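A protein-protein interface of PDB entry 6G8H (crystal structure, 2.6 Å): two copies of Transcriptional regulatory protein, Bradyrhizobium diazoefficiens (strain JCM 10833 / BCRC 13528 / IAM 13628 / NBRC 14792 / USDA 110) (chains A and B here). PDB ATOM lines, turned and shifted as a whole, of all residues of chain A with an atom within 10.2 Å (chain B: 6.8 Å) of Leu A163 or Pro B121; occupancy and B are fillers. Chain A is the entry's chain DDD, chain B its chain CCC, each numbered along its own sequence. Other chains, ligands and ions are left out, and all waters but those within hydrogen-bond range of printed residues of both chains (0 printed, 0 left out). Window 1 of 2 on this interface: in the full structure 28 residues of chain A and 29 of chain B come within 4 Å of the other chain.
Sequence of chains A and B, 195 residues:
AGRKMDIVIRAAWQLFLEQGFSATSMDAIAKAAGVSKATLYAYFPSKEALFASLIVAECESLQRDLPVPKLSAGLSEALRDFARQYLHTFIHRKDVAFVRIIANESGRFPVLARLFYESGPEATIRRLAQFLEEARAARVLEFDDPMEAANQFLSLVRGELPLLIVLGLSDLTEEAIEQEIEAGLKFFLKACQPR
1 position is printed for both chains.
Of the 6 pairs that touch across the chains among the printed residues, none has its exchanged pair printed and touching as well.
Hydrophobic or aromatic side chains of chain A that line the printed part of chain B: Leu A163, Leu A164 and Leu A167.
Hydrophobic or aromatic side chains of chain B that line the printed part of chain A: Phe B116, Tyr B117, Pro B121 and Ile B125.
Among the printed residues, 6 pairs touch across the chains.
Among the printed residues, no Asp or Glu carboxylate lies within 4 Å of a Lys or Arg side-chain nitrogen of the other chain.
The side-chain hydroxyl of Tyr B117 sits at hydrogen-bond distance from the side-chain carboxylate of Glu A160 (2.4 Å).
Pro B121 touches Glu A160 (CB to OE2, 3.6 Å).
OE1 of Glu A160 touches CD1 of Ile B125, 3.4 Å away.
Leu A163 touches Pro B121 (CD2 to CG, 3.8 Å).
Tyr B117 touches Leu A164.
Phe B116 touches Leu A167 (CD2 to CD1, 3.95 Å).
Leu A163 touches just one residue of chain B: Pro B121 (3.8 Å).
Of chain A, only Glu A160 (3.6 Å) and Leu A163 (3.8 Å) come within 4 Å of Pro B121.
No residue of chain A comes within 4 Å of Gly B120.
No residue of chain A comes within 4 Å of Thr B124.
Of the printed residues of chain A, Phe B116 touches Leu A167 (3.95 Å).
Printed residues of chain B within 4 Å of Leu A164: Tyr B117 (3.5 Å).
Printed residues of chain B within 4 Å of Leu A167: Phe B116.
Printed residues of chain A within 4 Å of Ile B125: Glu A160 (3.4 Å).
Of the printed residues of chain A, Tyr B117 touches Glu A160 and Leu A164.
Pro A162 touches none of the printed residues of chain B.
The nearest printed residue of chain B that does not touch Leu A167 is Val B99 (4.2 Å).
The backbone carbonyl oxygen of Tyr B117 lies within hydrogen-bond range of the backbone NH of Glu B122 (3.0 Å).
The backbone NH (N) of Leu A169 sits at hydrogen-bond distance from the backbone carbonyl oxygen (O) of Leu A164, 2.9 Å away.
The backbone carbonyl oxygen of Leu A164 sits at hydrogen-bond distance from the backbone NH of Ser A170 (3.4 Å).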
ATOM      1  N   PHE A  90      14.717  35.663   3.436  1.00  0.00           N
ATOM      2  CA  PHE A  90      15.740  34.634   3.174  1.00  0.00           C
ATOM      3  C   PHE A  90      15.154  33.416   2.488  1.00  0.00           C
ATOM      4  O   PHE A  90      15.722  32.935   1.500  1.00  0.00           O
ATOM      5  CB  PHE A  90      16.329  34.114   4.486  1.00  0.00           C
ATOM      6  CG  PHE A  90      17.789  34.382   4.509  1.00  0.00           C
ATOM      7  CD1 PHE A  90      18.624  33.680   3.679  1.00  0.00           C
ATOM      8  CD2 PHE A  90      18.280  35.457   5.212  1.00  0.00           C
ATOM      9  CE1 PHE A  90      19.959  34.021   3.595  1.00  0.00           C
ATOM     10  CE2 PHE A  90      19.614  35.793   5.129  1.00  0.00           C
ATOM     11  CZ  PHE A  90      20.454  35.063   4.333  1.00  0.00           C
ATOM     12  N   VAL A  96      19.920  34.011  -1.631  1.00  0.00           N
ATOM     13  CA  VAL A  96      20.799  32.819  -1.771  1.00  0.00           C
ATOM     14  C   VAL A  96      21.127  32.554  -3.248  1.00  0.00           C
ATOM     15  O   VAL A  96      22.298  32.195  -3.569  1.00  0.00           O
ATOM     16  CB  VAL A  96      20.165  31.610  -1.064  1.00  0.00           C
ATOM     17  CG1 VAL A  96      20.831  30.281  -1.414  1.00  0.00           C
ATOM     18  CG2 VAL A  96      20.215  31.851   0.436  1.00  0.00           C
ATOM     19  N   VAL A  99      23.748  35.022  -4.507  1.00  0.00           N
ATOM     20  CA  VAL A  99      25.073  34.701  -3.914  1.00  0.00           C
ATOM     21  C   VAL A  99      25.659  33.497  -4.638  1.00  0.00           C
ATOM     22  O   VAL A  99      26.867  33.456  -4.853  1.00  0.00           O
ATOM     23  CB  VAL A  99      24.928  34.458  -2.401  1.00  0.00           C
ATOM     24  CG1 VAL A  99      26.136  33.780  -1.803  1.00  0.00           C
ATOM     25  CG2 VAL A  99      24.578  35.750  -1.659  1.00  0.00           C
ATOM     26  N   ARG A 100      24.828  32.526  -4.981  1.00  0.00           N
ATOM     27  CA  ARG A 100      25.306  31.315  -5.688  1.00  0.00           C
ATOM     28  C   ARG A 100      25.855  31.785  -7.048  1.00  0.00           C
ATOM     29  O   ARG A 100      26.958  31.370  -7.433  1.00  0.00           O
ATOM     30  CB  ARG A 100      24.188  30.277  -5.796  1.00  0.00           C
ATOM     31  CG  ARG A 100      24.082  29.367  -4.580  1.00  0.00           C
ATOM     32  CD  ARG A 100      22.987  28.279  -4.728  1.00  0.00           C
ATOM     33  NE  ARG A 100      23.224  26.948  -5.296  1.00  0.00           N
ATOM     34  CZ  ARG A 100      24.426  26.382  -5.488  1.00  0.00           C
ATOM     35  NH1 ARG A 100      25.562  27.011  -5.201  1.00  0.00           N
ATOM     36  NH2 ARG A 100      24.494  25.164  -6.002  1.00  0.00           N
ATOM     37  N   ARG A 158      19.738  34.657  12.326  1.00  0.00           N
ATOM     38  CA  ARG A 158      20.023  33.920  11.071  1.00  0.00           C
ATOM     39  C   ARG A 158      20.687  32.572  11.392  1.00  0.00           C
ATOM     40  O   ARG A 158      20.387  31.561  10.720  1.00  0.00           O
ATOM     41  CB  ARG A 158      20.961  34.795  10.244  1.00  0.00           C
ATOM     42  CG  ARG A 158      21.222  34.300   8.839  1.00  0.00           C
ATOM     43  CD  ARG A 158      21.985  35.318   8.004  1.00  0.00           C
ATOM     44  NE  ARG A 158      23.352  35.556   8.424  1.00  0.00           N
ATOM     45  CZ  ARG A 158      23.813  36.747   8.825  1.00  0.00           C
ATOM     46  NH1 ARG A 158      23.038  37.813   8.830  1.00  0.00           N
ATOM     47  NH2 ARG A 158      25.061  36.899   9.189  1.00  0.00           N
ATOM     48  N   GLY A 159      21.616  32.546  12.350  1.00  0.00           N
ATOM     49  CA  GLY A 159      22.378  31.327  12.682  1.00  0.00           C
ATOM     50  C   GLY A 159      22.910  30.655  11.434  1.00  0.00           C
ATOM     51  O   GLY A 159      23.573  31.344  10.623  1.00  0.00           O
ATOM     52  N   GLU A 160      22.604  29.378  11.249  1.00  0.00           N
ATOM     53  CA  GLU A 160      23.214  28.549  10.173  1.00  0.00           C
ATOM     54  C   GLU A 160      22.270  28.357   8.976  1.00  0.00           C
ATOM     55  O   GLU A 160      22.582  27.563   8.079  1.00  0.00           O
ATOM     56  CB  GLU A 160      23.613  27.206  10.777  1.00  0.00           C
ATOM     57  CG  GLU A 160      25.123  27.054  10.904  1.00  0.00           C
ATOM     58  CD  GLU A 160      25.481  25.805  11.678  1.00  0.00           C
ATOM     59  OE1 GLU A 160      24.544  25.176  12.246  1.00  0.00           O
ATOM     60  OE2 GLU A 160      26.666  25.459  11.721  1.00  0.00           O
ATOM     61  N   LEU A 161      21.164  29.086   8.977  1.00  0.00           N
ATOM     62  CA  LEU A 161      20.058  28.956   8.028  1.00  0.00           C
ATOM     63  C   LEU A 161      20.548  29.055   6.590  1.00  0.00           C
ATOM     64  O   LEU A 161      20.152  28.272   5.742  1.00  0.00           O
ATOM     65  CB  LEU A 161      19.027  30.036   8.345  1.00  0.00           C
ATOM     66  CG  LEU A 161      17.943  30.152   7.303  1.00  0.00           C
ATOM     67  CD1 LEU A 161      17.195  28.834   7.201  1.00  0.00           C
ATOM     68  CD2 LEU A 161      17.009  31.286   7.638  1.00  0.00           C
ATOM     69  N   PRO A 162      21.400  30.017   6.212  1.00  0.00           N
ATOM     70  CA  PRO A 162      21.800  30.116   4.807  1.00  0.00           C
ATOM     71  C   PRO A 162      22.518  28.842   4.323  1.00  0.00           C
ATOM     72  O   PRO A 162      22.351  28.441   3.189  1.00  0.00           O
ATOM     73  CB  PRO A 162      22.720  31.340   4.781  1.00  0.00           C
ATOM     74  CG  PRO A 162      22.355  32.091   6.046  1.00  0.00           C
ATOM     75  CD  PRO A 162      22.024  31.034   7.075  1.00  0.00           C
ATOM     76  N   LEU A 163      23.306  28.223   5.186  1.00  0.00           N
ATOM     77  CA  LEU A 163      23.989  26.945   4.827  1.00  0.00           C
ATOM     78  C   LEU A 163      22.951  25.825   4.708  1.00  0.00           C
ATOM     79  O   LEU A 163      23.021  25.053   3.767  1.00  0.00           O
ATOM     80  CB  LEU A 163      25.069  26.591   5.863  1.00  0.00           C
ATOM     81  CG  LEU A 163      25.798  25.263   5.616  1.00  0.00           C
ATOM     82  CD1 LEU A 163      26.550  25.211   4.298  1.00  0.00           C
ATOM     83  CD2 LEU A 163      26.790  24.991   6.731  1.00  0.00           C
ATOM     84  N   LEU A 164      22.031  25.714   5.652  1.00  0.00           N
ATOM     85  CA  LEU A 164      20.938  24.696   5.588  1.00  0.00           C
ATOM     86  C   LEU A 164      20.167  24.875   4.265  1.00  0.00           C
ATOM     87  O   LEU A 164      19.947  23.884   3.579  1.00  0.00           O
ATOM     88  CB  LEU A 164      20.057  24.826   6.838  1.00  0.00           C
ATOM     89  CG  LEU A 164      20.733  24.499   8.169  1.00  0.00           C
ATOM     90  CD1 LEU A 164      19.863  24.850   9.346  1.00  0.00           C
ATOM     91  CD2 LEU A 164      21.098  23.062   8.247  1.00  0.00           C
ATOM     92  N   ILE A 165      19.913  26.104   3.832  1.00  0.00           N
ATOM     93  CA  ILE A 165      19.098  26.375   2.614  1.00  0.00           C
ATOM     94  C   ILE A 165      19.871  25.877   1.405  1.00  0.00           C
ATOM     95  O   ILE A 165      19.315  25.132   0.602  1.00  0.00           O
ATOM     96  CB  ILE A 165      18.722  27.866   2.491  1.00  0.00           C
ATOM     97  CG1 ILE A 165      17.685  28.252   3.548  1.00  0.00           C
ATOM     98  CG2 ILE A 165      18.258  28.212   1.081  1.00  0.00           C
ATOM     99  CD1 ILE A 165      17.597  29.739   3.777  1.00  0.00           C
ATOM    100  N   VAL A 166      21.130  26.257   1.315  1.00  0.00           N
ATOM    101  CA  VAL A 166      22.029  25.909   0.184  1.00  0.00           C
ATOM    102  C   VAL A 166      22.211  24.380   0.107  1.00  0.00           C
ATOM    103  O   VAL A 166      22.327  23.841  -0.982  1.00  0.00           O
ATOM    104  CB  VAL A 166      23.334  26.692   0.390  1.00  0.00           C
ATOM    105  CG1 VAL A 166      24.567  25.871   0.141  1.00  0.00           C
ATOM    106  CG2 VAL A 166      23.357  27.923  -0.447  1.00  0.00           C
ATOM    107  N   LEU A 167      22.216  23.677   1.230  1.00  0.00           N
ATOM    108  CA  LEU A 167      22.356  22.194   1.276  1.00  0.00           C
ATOM    109  C   LEU A 167      20.998  21.513   1.033  1.00  0.00           C
ATOM    110  O   LEU A 167      20.945  20.304   1.089  1.00  0.00           O
ATOM    111  CB  LEU A 167      22.902  21.788   2.643  1.00  0.00           C
ATOM    112  CG  LEU A 167      24.355  22.173   2.921  1.00  0.00           C
ATOM    113  CD1 LEU A 167      24.786  21.732   4.315  1.00  0.00           C
ATOM    114  CD2 LEU A 167      25.301  21.597   1.888  1.00  0.00           C
ATOM    115  N   GLY A 168      19.922  22.269   0.837  1.00  0.00           N
ATOM    116  CA  GLY A 168      18.561  21.725   0.679  1.00  0.00           C
ATOM    117  C   GLY A 168      17.989  21.111   1.940  1.00  0.00           C
ATOM    118  O   GLY A 168      17.165  20.265   1.804  1.00  0.00           O
ATOM    119  N   LEU A 169      18.350  21.539   3.138  1.00  0.00           N
ATOM    120  CA  LEU A 169      17.914  20.915   4.405  1.00  0.00           C
ATOM    121  C   LEU A 169      17.201  21.939   5.278  1.00  0.00           C
ATOM    122  O   LEU A 169      17.066  21.699   6.526  1.00  0.00           O
ATOM    123  CB  LEU A 169      19.124  20.447   5.217  1.00  0.00           C
ATOM    124  CG  LEU A 169      20.133  19.541   4.548  1.00  0.00           C
ATOM    125  CD1 LEU A 169      21.287  19.335   5.492  1.00  0.00           C
ATOM    126  CD2 LEU A 169      19.480  18.225   4.181  1.00  0.00           C
ATOM    127  N   SER A 170      16.838  23.094   4.751  1.00  0.00           N
ATOM    128  CA  SER A 170      15.976  24.018   5.527  1.00  0.00           C
ATOM    129  C   SER A 170      14.520  23.806   5.139  1.00  0.00           C
ATOM    130  O   SER A 170      14.181  24.019   3.962  1.00  0.00           O
ATOM    131  CB  SER A 170      16.339  25.428   5.398  1.00  0.00           C
ATOM    132  OG  SER A 170      15.588  26.081   6.409  1.00  0.00           O
ATOM    133  N   ASP A 171      13.758  23.307   6.094  1.00  0.00           N
ATOM    134  CA  ASP A 171      12.394  22.777   5.898  1.00  0.00           C
ATOM    135  C   ASP A 171      11.688  23.053   7.221  1.00  0.00           C
ATOM    136  O   ASP A 171      11.301  22.134   7.944  1.00  0.00           O
ATOM    137  CB  ASP A 171      12.460  21.308   5.485  1.00  0.00           C
ATOM    138  CG  ASP A 171      11.094  20.757   5.175  1.00  0.00           C
ATOM    139  OD1 ASP A 171      10.285  21.527   4.616  1.00  0.00           O
ATOM    140  OD2 ASP A 171      10.843  19.592   5.547  1.00  0.00           O
ATOM    141  N   LEU A 172      11.699  24.320   7.614  1.00  0.00           N
ATOM    142  CA  LEU A 172      11.409  24.773   9.000  1.00  0.00           C
ATOM    143  C   LEU A 172      10.049  25.462   8.965  1.00  0.00           C
ATOM    144  O   LEU A 172       9.871  26.425   8.205  1.00  0.00           O
ATOM    145  CB  LEU A 172      12.545  25.683   9.492  1.00  0.00           C
ATOM    146  CG  LEU A 172      13.867  24.952   9.801  1.00  0.00           C
ATOM    147  CD1 LEU A 172      15.091  25.857   9.653  1.00  0.00           C
ATOM    148  CD2 LEU A 172      13.828  24.276  11.169  1.00  0.00           C
ATOM    149  N   CYS B  59      35.421  15.197   6.596  1.00  0.00           N
ATOM    150  CA  CYS B  59      34.935  15.902   7.804  1.00  0.00           C
ATOM    151  C   CYS B  59      35.759  15.504   9.033  1.00  0.00           C
ATOM    152  O   CYS B  59      35.936  16.375   9.855  1.00  0.00           O
ATOM    153  CB  CYS B  59      33.450  15.660   8.034  1.00  0.00           C
ATOM    154  SG  CYS B  59      32.420  16.439   6.777  1.00  0.00           S
ATOM    155  N   GLN B  63      37.995  18.296  11.054  1.00  0.00           N
ATOM    156  CA  GLN B  63      37.760  18.356  12.515  1.00  0.00           C
ATOM    157  C   GLN B  63      39.094  18.237  13.266  1.00  0.00           C
ATOM    158  O   GLN B  63      39.140  18.687  14.387  1.00  0.00           O
ATOM    159  CB  GLN B  63      36.765  17.269  12.931  1.00  0.00           C
ATOM    160  CG  GLN B  63      35.338  17.663  12.622  1.00  0.00           C
ATOM    161  CD  GLN B  63      34.813  18.559  13.709  1.00  0.00           C
ATOM    162  OE1 GLN B  63      34.778  18.166  14.899  1.00  0.00           O
ATOM    163  NE2 GLN B  63      34.298  19.713  13.280  1.00  0.00           N
ATOM    164  N   TYR B  86      38.668  28.361  13.716  1.00  0.00           N
ATOM    165  CA  TYR B  86      37.356  28.223  13.051  1.00  0.00           C
ATOM    166  C   TYR B  86      37.269  29.138  11.838  1.00  0.00           C
ATOM    167  O   TYR B  86      36.849  28.689  10.785  1.00  0.00           O
ATOM    168  CB  TYR B  86      36.256  28.561  14.045  1.00  0.00           C
ATOM    169  CG  TYR B  86      34.867  28.569  13.482  1.00  0.00           C
ATOM    170  CD1 TYR B  86      34.345  27.430  12.921  1.00  0.00           C
ATOM    171  CD2 TYR B  86      34.060  29.691  13.594  1.00  0.00           C
ATOM    172  CE1 TYR B  86      33.030  27.390  12.482  1.00  0.00           C
ATOM    173  CE2 TYR B  86      32.753  29.674  13.142  1.00  0.00           C
ATOM    174  CZ  TYR B  86      32.224  28.512  12.591  1.00  0.00           C
ATOM    175  OH  TYR B  86      30.942  28.470  12.125  1.00  0.00           O
ATOM    176  N   ASP B  95      35.788  24.014   3.125  1.00  0.00           N
ATOM    177  CA  ASP B  95      34.475  23.327   3.009  1.00  0.00           C
ATOM    178  C   ASP B  95      33.988  23.518   1.561  1.00  0.00           C
ATOM    179  O   ASP B  95      33.111  22.768   1.143  1.00  0.00           O
ATOM    180  CB  ASP B  95      33.480  23.821   4.085  1.00  0.00           C
ATOM    181  CG  ASP B  95      33.382  22.954   5.349  1.00  0.00           C
ATOM    182  OD1 ASP B  95      33.879  21.795   5.359  1.00  0.00           O
ATOM    183  OD2 ASP B  95      32.757  23.413   6.329  1.00  0.00           O
ATOM    184  N   VAL B  99      30.884  21.455  -0.484  1.00  0.00           N
ATOM    185  CA  VAL B  99      29.534  22.063  -0.379  1.00  0.00           C
ATOM    186  C   VAL B  99      29.053  22.369  -1.794  1.00  0.00           C
ATOM    187  O   VAL B  99      27.848  22.294  -2.039  1.00  0.00           O
ATOM    188  CB  VAL B  99      29.575  23.322   0.496  1.00  0.00           C
ATOM    189  CG1 VAL B  99      28.323  24.156   0.379  1.00  0.00           C
ATOM    190  CG2 VAL B  99      29.846  23.011   1.952  1.00  0.00           C
ATOM    191  N   PHE B 116      26.826  15.296   5.683  1.00  0.00           N
ATOM    192  CA  PHE B 116      27.840  16.368   5.624  1.00  0.00           C
ATOM    193  C   PHE B 116      27.564  17.365   6.757  1.00  0.00           C
ATOM    194  O   PHE B 116      28.485  17.699   7.522  1.00  0.00           O
ATOM    195  CB  PHE B 116      27.880  17.067   4.268  1.00  0.00           C
ATOM    196  CG  PHE B 116      28.697  18.322   4.354  1.00  0.00           C
ATOM    197  CD1 PHE B 116      30.081  18.262   4.392  1.00  0.00           C
ATOM    198  CD2 PHE B 116      28.079  19.553   4.532  1.00  0.00           C
ATOM    199  CE1 PHE B 116      30.824  19.414   4.569  1.00  0.00           C
ATOM    200  CE2 PHE B 116      28.830  20.706   4.703  1.00  0.00           C
ATOM    201  CZ  PHE B 116      30.200  20.631   4.725  1.00  0.00           C
ATOM    202  N   TYR B 117      26.325  17.810   6.906  1.00  0.00           N
ATOM    203  CA  TYR B 117      25.991  18.814   7.943  1.00  0.00           C
ATOM    204  C   TYR B 117      26.367  18.271   9.331  1.00  0.00           C
ATOM    205  O   TYR B 117      27.044  18.970  10.059  1.00  0.00           O
ATOM    206  CB  TYR B 117      24.538  19.261   7.829  1.00  0.00           C
ATOM    207  CG  TYR B 117      24.187  20.287   8.863  1.00  0.00           C
ATOM    208  CD1 TYR B 117      24.595  21.610   8.708  1.00  0.00           C
ATOM    209  CD2 TYR B 117      23.563  19.916  10.049  1.00  0.00           C
ATOM    210  CE1 TYR B 117      24.280  22.563   9.663  1.00  0.00           C
ATOM    211  CE2 TYR B 117      23.326  20.838  11.055  1.00  0.00           C
ATOM    212  CZ  TYR B 117      23.642  22.171  10.835  1.00  0.00           C
ATOM    213  OH  TYR B 117      23.365  23.075  11.815  1.00  0.00           O
ATOM    214  N   GLU B 118      25.992  17.046   9.669  1.00  0.00           N
ATOM    215  CA  GLU B 118      26.153  16.457  11.031  1.00  0.00           C
ATOM    216  C   GLU B 118      27.625  16.116  11.284  1.00  0.00           C
ATOM    217  O   GLU B 118      28.060  16.222  12.408  1.00  0.00           O
ATOM    218  CB  GLU B 118      25.211  15.265  11.284  1.00  0.00           C
ATOM    219  CG  GLU B 118      23.744  15.661  11.130  1.00  0.00           C
ATOM    220  CD  GLU B 118      22.667  14.918  11.901  1.00  0.00           C
ATOM    221  OE1 GLU B 118      22.900  13.732  12.185  1.00  0.00           O
ATOM    222  OE2 GLU B 118      21.637  15.590  12.269  1.00  0.00           O
ATOM    223  N   SER B 119      28.380  15.724  10.273  1.00  0.00           N
ATOM    224  CA  SER B 119      29.814  15.317  10.388  1.00  0.00           C
ATOM    225  C   SER B 119      30.750  16.544  10.423  1.00  0.00           C
ATOM    226  O   SER B 119      31.891  16.420  10.847  1.00  0.00           O
ATOM    227  CB  SER B 119      30.184  14.428   9.249  1.00  0.00           C
ATOM    228  OG  SER B 119      29.363  13.295   9.213  1.00  0.00           O
ATOM    229  N   GLY B 120      30.311  17.685   9.901  1.00  0.00           N
ATOM    230  CA  GLY B 120      31.105  18.916   9.812  1.00  0.00           C
ATOM    231  C   GLY B 120      30.531  20.010  10.707  1.00  0.00           C
ATOM    232  O   GLY B 120      30.817  20.089  11.902  1.00  0.00           O
ATOM    233  N   PRO B 121      29.774  20.963  10.147  1.00  0.00           N
ATOM    234  CA  PRO B 121      29.299  22.114  10.929  1.00  0.00           C
ATOM    235  C   PRO B 121      28.646  21.771  12.273  1.00  0.00           C
ATOM    236  O   PRO B 121      28.943  22.436  13.241  1.00  0.00           O
ATOM    237  CB  PRO B 121      28.249  22.745  10.016  1.00  0.00           C
ATOM    238  CG  PRO B 121      28.745  22.373   8.612  1.00  0.00           C
ATOM    239  CD  PRO B 121      29.394  21.004   8.731  1.00  0.00           C
ATOM    240  N   GLU B 122      27.771  20.761  12.331  1.00  0.00           N
ATOM    241  CA  GLU B 122      27.137  20.376  13.610  1.00  0.00           C
ATOM    242  C   GLU B 122      28.190  19.734  14.528  1.00  0.00           C
ATOM    243  O   GLU B 122      28.088  19.904  15.735  1.00  0.00           O
ATOM    244  CB  GLU B 122      25.916  19.483  13.396  1.00  0.00           C
ATOM    245  CG  GLU B 122      24.999  19.508  14.589  1.00  0.00           C
ATOM    246  CD  GLU B 122      23.606  18.937  14.372  1.00  0.00           C
ATOM    247  OE1 GLU B 122      22.631  19.747  14.197  1.00  0.00           O
ATOM    248  OE2 GLU B 122      23.483  17.682  14.469  1.00  0.00           O
ATOM    249  N   ALA B 123      29.188  19.023  14.011  1.00  0.00           N
ATOM    250  CA  ALA B 123      30.296  18.438  14.823  1.00  0.00           C
ATOM    251  C   ALA B 123      31.060  19.556  15.532  1.00  0.00           C
ATOM    252  O   ALA B 123      31.362  19.389  16.738  1.00  0.00           O
ATOM    253  CB  ALA B 123      31.235  17.591  13.995  1.00  0.00           C
ATOM    254  N   THR B 124      31.328  20.657  14.841  1.00  0.00           N
ATOM    255  CA  THR B 124      31.982  21.862  15.420  1.00  0.00           C
ATOM    256  C   THR B 124      31.126  22.427  16.562  1.00  0.00           C
ATOM    257  O   THR B 124      31.664  22.736  17.623  1.00  0.00           O
ATOM    258  CB  THR B 124      32.245  22.932  14.356  1.00  0.00           C
ATOM    259  OG1 THR B 124      33.105  22.412  13.347  1.00  0.00           O
ATOM    260  CG2 THR B 124      32.867  24.177  14.931  1.00  0.00           C
ATOM    261  N   ILE B 125      29.821  22.520  16.374  1.00  0.00           N
ATOM    262  CA  ILE B 125      28.899  22.990  17.451  1.00  0.00           C
ATOM    263  C   ILE B 125      29.005  22.049  18.653  1.00  0.00           C
ATOM    264  O   ILE B 125      29.146  22.554  19.778  1.00  0.00           O
ATOM    265  CB  ILE B 125      27.462  23.115  16.902  1.00  0.00           C
ATOM    266  CG1 ILE B 125      27.360  24.188  15.813  1.00  0.00           C
ATOM    267  CG2 ILE B 125      26.444  23.351  18.001  1.00  0.00           C
ATOM    268  CD1 ILE B 125      26.047  24.168  15.075  1.00  0.00           C
ATOM    269  N   ARG B 126      28.960  20.728  18.446  1.00  0.00           N
ATOM    270  CA  ARG B 126      28.958  19.722  19.545  1.00  0.00           C
ATOM    271  C   ARG B 126      30.271  19.803  20.319  1.00  0.00           C
ATOM    272  O   ARG B 126      30.182  19.822  21.570  1.00  0.00           O
ATOM    273  CB  ARG B 126      28.689  18.310  19.031  1.00  0.00           C
ATOM    274  CG  ARG B 126      27.263  18.139  18.510  1.00  0.00           C
ATOM    275  CD  ARG B 126      26.876  16.709  18.170  1.00  0.00           C
ATOM    276  NE  ARG B 126      27.769  16.078  17.192  1.00  0.00           N
ATOM    277  CZ  ARG B 126      27.582  16.047  15.855  1.00  0.00           C
ATOM    278  NH1 ARG B 126      26.500  16.562  15.277  1.00  0.00           N
ATOM    279  NH2 ARG B 126      28.491  15.465  15.090  1.00  0.00           N
ATOM    280  N   LEU B 154      29.479  30.897  17.714  1.00  0.00           N
ATOM    281  CA  LEU B 154      30.011  30.694  16.346  1.00  0.00           C
ATOM    282  C   LEU B 154      29.354  31.698  15.404  1.00  0.00           C
ATOM    283  O   LEU B 154      30.060  32.282  14.601  1.00  0.00           O
ATOM    284  CB  LEU B 154      29.786  29.242  15.917  1.00  0.00           C
ATOM    285  CG  LEU B 154      30.608  28.202  16.690  1.00  0.00           C
ATOM    286  CD1 LEU B 154      30.239  26.796  16.223  1.00  0.00           C
ATOM    287  CD2 LEU B 154      32.118  28.440  16.547  1.00  0.00           C
